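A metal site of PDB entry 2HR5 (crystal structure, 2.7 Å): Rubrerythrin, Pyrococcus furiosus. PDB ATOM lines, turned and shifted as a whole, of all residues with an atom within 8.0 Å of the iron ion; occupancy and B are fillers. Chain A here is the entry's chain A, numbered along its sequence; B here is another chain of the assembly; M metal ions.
The iron ion is bound by SG of Cys 142 (2.2 Å), SG of Cys 157 (2.3 Å), SG of Cys 160 (2.3 Å) and SG of Cys 145 (2.3 Å). The iron ion has four donor atoms within binding distance.
Four residues have an atom within 4 Å of the iron ion: Cys 142, Cys 145, Cys 157 and Cys 160. Along chain A the residues within 4 Å of the iron ion span positions 142 to 160.
The backbone NH (N) of Ile 144 lies close to the side-chain sulfur (SG) of Cys 142 (3.6 Å). O of Tyr 147 lies within hydrogen-bond range of N of Cys 142, at 2.8 Å. The backbone NH of Cys 157 is in hydrogen-bond range of the backbone carbonyl oxygen of Ala 162, 2.8 Å away. The side-chain sulfur of Cys 157 lies close to the backbone NH of Val 159 (3.3 Å). The side-chain sulfur (SG) of Cys 160 sits close to the backbone NH (N) of Ala 162 (3.7 Å). The backbone NH (N) of Tyr 147 lies close to the side-chain sulfur (SG) of Cys 145, at 3.4 Å.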
ATOM      1  N   TYR A 109      15.904  -3.243 -22.241  1.00  0.00           N
ATOM      2  CA  TYR A 109      16.291  -4.649 -22.187  1.00  0.00           C
ATOM      3  C   TYR A 109      17.702  -4.810 -21.659  1.00  0.00           C
ATOM      4  O   TYR A 109      17.870  -5.399 -20.648  1.00  0.00           O
ATOM      5  CB  TYR A 109      16.106  -5.426 -23.522  1.00  0.00           C
ATOM      6  CG  TYR A 109      14.682  -5.723 -23.937  1.00  0.00           C
ATOM      7  CD1 TYR A 109      13.593  -5.485 -23.088  1.00  0.00           C
ATOM      8  CD2 TYR A 109      14.408  -6.264 -25.214  1.00  0.00           C
ATOM      9  CE1 TYR A 109      12.323  -5.762 -23.500  1.00  0.00           C
ATOM     10  CE2 TYR A 109      13.132  -6.561 -25.635  1.00  0.00           C
ATOM     11  CZ  TYR A 109      12.098  -6.325 -24.771  1.00  0.00           C
ATOM     12  OH  TYR A 109      10.806  -6.621 -25.218  1.00  0.00           O
ATOM     13  N   ILE A 141      19.517 -17.698 -20.079  1.00  0.00           N
ATOM     14  CA  ILE A 141      19.534 -16.404 -20.661  1.00  0.00           C
ATOM     15  C   ILE A 141      18.269 -16.236 -21.494  1.00  0.00           C
ATOM     16  O   ILE A 141      18.013 -17.053 -22.371  1.00  0.00           O
ATOM     17  CB  ILE A 141      20.765 -16.252 -21.630  1.00  0.00           C
ATOM     18  CG1 ILE A 141      22.092 -16.768 -21.026  1.00  0.00           C
ATOM     19  CG2 ILE A 141      20.830 -14.841 -22.202  1.00  0.00           C
ATOM     20  CD1 ILE A 141      22.562 -16.039 -19.732  1.00  0.00           C
ATOM     21  N   CYS A 142      17.492 -15.193 -21.260  1.00  0.00           N
ATOM     22  CA  CYS A 142      16.340 -14.931 -22.110  1.00  0.00           C
ATOM     23  C   CYS A 142      16.757 -14.414 -23.522  1.00  0.00           C
ATOM     24  O   CYS A 142      17.492 -13.419 -23.614  1.00  0.00           O
ATOM     25  CB  CYS A 142      15.455 -13.916 -21.442  1.00  0.00           C
ATOM     26  SG  CYS A 142      14.145 -13.347 -22.460  1.00  0.00           S
ATOM     27  N   PRO A 143      16.294 -15.091 -24.611  1.00  0.00           N
ATOM     28  CA  PRO A 143      16.874 -14.762 -25.880  1.00  0.00           C
ATOM     29  C   PRO A 143      16.205 -13.577 -26.550  1.00  0.00           C
ATOM     30  O   PRO A 143      16.548 -13.292 -27.704  1.00  0.00           O
ATOM     31  CB  PRO A 143      16.697 -16.044 -26.686  1.00  0.00           C
ATOM     32  CG  PRO A 143      15.375 -16.567 -26.205  1.00  0.00           C
ATOM     33  CD  PRO A 143      15.331 -16.205 -24.736  1.00  0.00           C
ATOM     34  N   ILE A 144      15.262 -12.938 -25.857  1.00  0.00           N
ATOM     35  CA  ILE A 144      14.595 -11.720 -26.308  1.00  0.00           C
ATOM     36  C   ILE A 144      15.277 -10.473 -25.727  1.00  0.00           C
ATOM     37  O   ILE A 144      15.446  -9.440 -26.415  1.00  0.00           O
ATOM     38  CB  ILE A 144      13.135 -11.703 -25.792  1.00  0.00           C
ATOM     39  CG1 ILE A 144      12.435 -12.997 -26.179  1.00  0.00           C
ATOM     40  CG2 ILE A 144      12.365 -10.489 -26.299  1.00  0.00           C
ATOM     41  CD1 ILE A 144      12.334 -13.240 -27.654  1.00  0.00           C
ATOM     42  N   CYS A 145      15.661 -10.540 -24.448  1.00  0.00           N
ATOM     43  CA  CYS A 145      16.101  -9.376 -23.716  1.00  0.00           C
ATOM     44  C   CYS A 145      17.420  -9.670 -23.033  1.00  0.00           C
ATOM     45  O   CYS A 145      18.110  -8.765 -22.615  1.00  0.00           O
ATOM     46  CB  CYS A 145      15.041  -8.916 -22.705  1.00  0.00           C
ATOM     47  SG  CYS A 145      14.900  -9.951 -21.234  1.00  0.00           S
ATOM     48  N   GLY A 146      17.814 -10.915 -22.945  1.00  0.00           N
ATOM     49  CA  GLY A 146      19.098 -11.167 -22.287  1.00  0.00           C
ATOM     50  C   GLY A 146      19.079 -11.167 -20.771  1.00  0.00           C
ATOM     51  O   GLY A 146      20.121 -11.274 -20.188  1.00  0.00           O
ATOM     52  N   TYR A 147      17.910 -11.056 -20.144  1.00  0.00           N
ATOM     53  CA  TYR A 147      17.779 -11.330 -18.708  1.00  0.00           C
ATOM     54  C   TYR A 147      18.594 -12.580 -18.436  1.00  0.00           C
ATOM     55  O   TYR A 147      18.546 -13.529 -19.218  1.00  0.00           O
ATOM     56  CB  TYR A 147      16.270 -11.552 -18.285  1.00  0.00           C
ATOM     57  CG  TYR A 147      16.070 -12.244 -16.957  1.00  0.00           C
ATOM     58  CD1 TYR A 147      15.908 -13.645 -16.849  1.00  0.00           C
ATOM     59  CD2 TYR A 147      16.097 -11.519 -15.786  1.00  0.00           C
ATOM     60  CE1 TYR A 147      15.728 -14.269 -15.555  1.00  0.00           C
ATOM     61  CE2 TYR A 147      15.954 -12.115 -14.512  1.00  0.00           C
ATOM     62  CZ  TYR A 147      15.773 -13.456 -14.404  1.00  0.00           C
ATOM     63  OH  TYR A 147      15.616 -13.911 -13.130  1.00  0.00           O
ATOM     64  N   THR A 148      19.283 -12.578 -17.298  1.00  0.00           N
ATOM     65  CA  THR A 148      20.238 -13.625 -16.930  1.00  0.00           C
ATOM     66  C   THR A 148      19.979 -14.071 -15.493  1.00  0.00           C
ATOM     67  O   THR A 148      19.743 -13.234 -14.607  1.00  0.00           O
ATOM     68  CB  THR A 148      21.630 -13.051 -16.999  1.00  0.00           C
ATOM     69  OG1 THR A 148      21.767 -12.455 -18.304  1.00  0.00           O
ATOM     70  CG2 THR A 148      22.716 -14.127 -16.720  1.00  0.00           C
ATOM     71  N   TYR A 156       8.562 -16.965 -15.919  1.00  0.00           N
ATOM     72  CA  TYR A 156       8.566 -16.048 -17.093  1.00  0.00           C
ATOM     73  C   TYR A 156       9.668 -15.022 -16.878  1.00  0.00           C
ATOM     74  O   TYR A 156       9.929 -14.693 -15.737  1.00  0.00           O
ATOM     75  CB  TYR A 156       7.207 -15.325 -17.279  1.00  0.00           C
ATOM     76  CG  TYR A 156       6.082 -16.280 -17.503  1.00  0.00           C
ATOM     77  CD1 TYR A 156       5.708 -16.674 -18.810  1.00  0.00           C
ATOM     78  CD2 TYR A 156       5.425 -16.866 -16.392  1.00  0.00           C
ATOM     79  CE1 TYR A 156       4.703 -17.596 -19.010  1.00  0.00           C
ATOM     80  CE2 TYR A 156       4.425 -17.789 -16.584  1.00  0.00           C
ATOM     81  CZ  TYR A 156       4.060 -18.143 -17.861  1.00  0.00           C
ATOM     82  OH  TYR A 156       3.039 -19.033 -17.993  1.00  0.00           O
ATOM     83  N   CYS A 157      10.324 -14.555 -17.956  1.00  0.00           N
ATOM     84  CA  CYS A 157      11.296 -13.451 -17.814  1.00  0.00           C
ATOM     85  C   CYS A 157      10.656 -12.221 -17.168  1.00  0.00           C
ATOM     86  O   CYS A 157       9.588 -11.750 -17.623  1.00  0.00           O
ATOM     87  CB  CYS A 157      11.894 -13.105 -19.173  1.00  0.00           C
ATOM     88  SG  CYS A 157      12.926 -11.687 -19.244  1.00  0.00           S
ATOM     89  N   PRO A 158      11.283 -11.705 -16.098  1.00  0.00           N
ATOM     90  CA  PRO A 158      10.632 -10.604 -15.437  1.00  0.00           C
ATOM     91  C   PRO A 158      10.748  -9.320 -16.285  1.00  0.00           C
ATOM     92  O   PRO A 158      10.129  -8.305 -15.936  1.00  0.00           O
ATOM     93  CB  PRO A 158      11.388 -10.474 -14.081  1.00  0.00           C
ATOM     94  CG  PRO A 158      12.647 -11.065 -14.238  1.00  0.00           C
ATOM     95  CD  PRO A 158      12.529 -12.095 -15.409  1.00  0.00           C
ATOM     96  N   VAL A 159      11.532  -9.362 -17.380  1.00  0.00           N
ATOM     97  CA  VAL A 159      11.646  -8.168 -18.241  1.00  0.00           C
ATOM     98  C   VAL A 159      10.666  -8.133 -19.463  1.00  0.00           C
ATOM     99  O   VAL A 159       9.968  -7.150 -19.682  1.00  0.00           O
ATOM    100  CB  VAL A 159      13.128  -7.853 -18.542  1.00  0.00           C
ATOM    101  CG1 VAL A 159      13.263  -6.772 -19.591  1.00  0.00           C
ATOM    102  CG2 VAL A 159      13.760  -7.405 -17.256  1.00  0.00           C
ATOM    103  N   CYS A 160      10.643  -9.183 -20.251  1.00  0.00           N
ATOM    104  CA  CYS A 160       9.789  -9.115 -21.383  1.00  0.00           C
ATOM    105  C   CYS A 160       8.637 -10.083 -21.232  1.00  0.00           C
ATOM    106  O   CYS A 160       7.773 -10.091 -22.095  1.00  0.00           O
ATOM    107  CB  CYS A 160      10.578  -9.390 -22.660  1.00  0.00           C
ATOM    108  SG  CYS A 160      11.373 -11.003 -22.676  1.00  0.00           S
ATOM    109  N   GLY A 161       8.614 -10.940 -20.197  1.00  0.00           N
ATOM    110  CA  GLY A 161       7.536 -12.005 -20.149  1.00  0.00           C
ATOM    111  C   GLY A 161       7.681 -13.327 -20.994  1.00  0.00           C
ATOM    112  O   GLY A 161       6.805 -14.175 -21.001  1.00  0.00           O
ATOM    113  N   ALA A 162       8.805 -13.486 -21.711  1.00  0.00           N
ATOM    114  CA  ALA A 162       9.149 -14.729 -22.404  1.00  0.00           C
ATOM    115  C   ALA A 162       9.030 -15.902 -21.436  1.00  0.00           C
ATOM    116  O   ALA A 162       9.402 -15.770 -20.260  1.00  0.00           O
ATOM    117  CB  ALA A 162      10.569 -14.644 -22.964  1.00  0.00           C
ATOM    118  N   PRO A 163       8.423 -17.022 -21.884  1.00  0.00           N
ATOM    119  CA  PRO A 163       8.340 -18.157 -20.959  1.00  0.00           C
ATOM    120  C   PRO A 163       9.696 -18.830 -20.724  1.00  0.00           C
ATOM    121  O   PRO A 163      10.547 -18.804 -21.613  1.00  0.00           O
ATOM    122  CB  PRO A 163       7.291 -19.083 -21.631  1.00  0.00           C
ATOM    123  CG  PRO A 163       7.234 -18.727 -23.060  1.00  0.00           C
ATOM    124  CD  PRO A 163       7.666 -17.272 -23.150  1.00  0.00           C
ATOM    125  N   PHE A 167      14.187 -20.055 -22.642  1.00  0.00           N
ATOM    126  CA  PHE A 167      15.512 -19.630 -22.154  1.00  0.00           C
ATOM    127  C   PHE A 167      16.690 -20.412 -22.744  1.00  0.00           C
ATOM    128  O   PHE A 167      16.562 -21.560 -22.986  1.00  0.00           O
ATOM    129  CB  PHE A 167      15.631 -19.648 -20.638  1.00  0.00           C
ATOM    130  CG  PHE A 167      14.722 -18.641 -19.911  1.00  0.00           C
ATOM    131  CD1 PHE A 167      13.960 -17.710 -20.590  1.00  0.00           C
ATOM    132  CD2 PHE A 167      14.669 -18.640 -18.513  1.00  0.00           C
ATOM    133  CE1 PHE A 167      13.165 -16.790 -19.897  1.00  0.00           C
ATOM    134  CE2 PHE A 167      13.880 -17.720 -17.788  1.00  0.00           C
ATOM    135  CZ  PHE A 167      13.127 -16.790 -18.473  1.00  0.00           C
ATOM    136  N   VAL B  54      22.536 -11.057 -27.554  1.00  0.00           N
ATOM    137  CA  VAL B  54      21.123 -10.689 -27.613  1.00  0.00           C
ATOM    138  C   VAL B  54      20.908  -9.163 -27.626  1.00  0.00           C
ATOM    139  O   VAL B  54      20.079  -8.611 -28.414  1.00  0.00           O
ATOM    140  CB  VAL B  54      20.310 -11.426 -26.473  1.00  0.00           C
ATOM    141  CG1 VAL B  54      18.970 -10.809 -26.279  1.00  0.00           C
ATOM    142  CG2 VAL B  54      20.107 -12.890 -26.806  1.00  0.00           C
HETATM  143 FE    FE M   1      13.231 -11.544 -21.479  1.00  0.00          FE
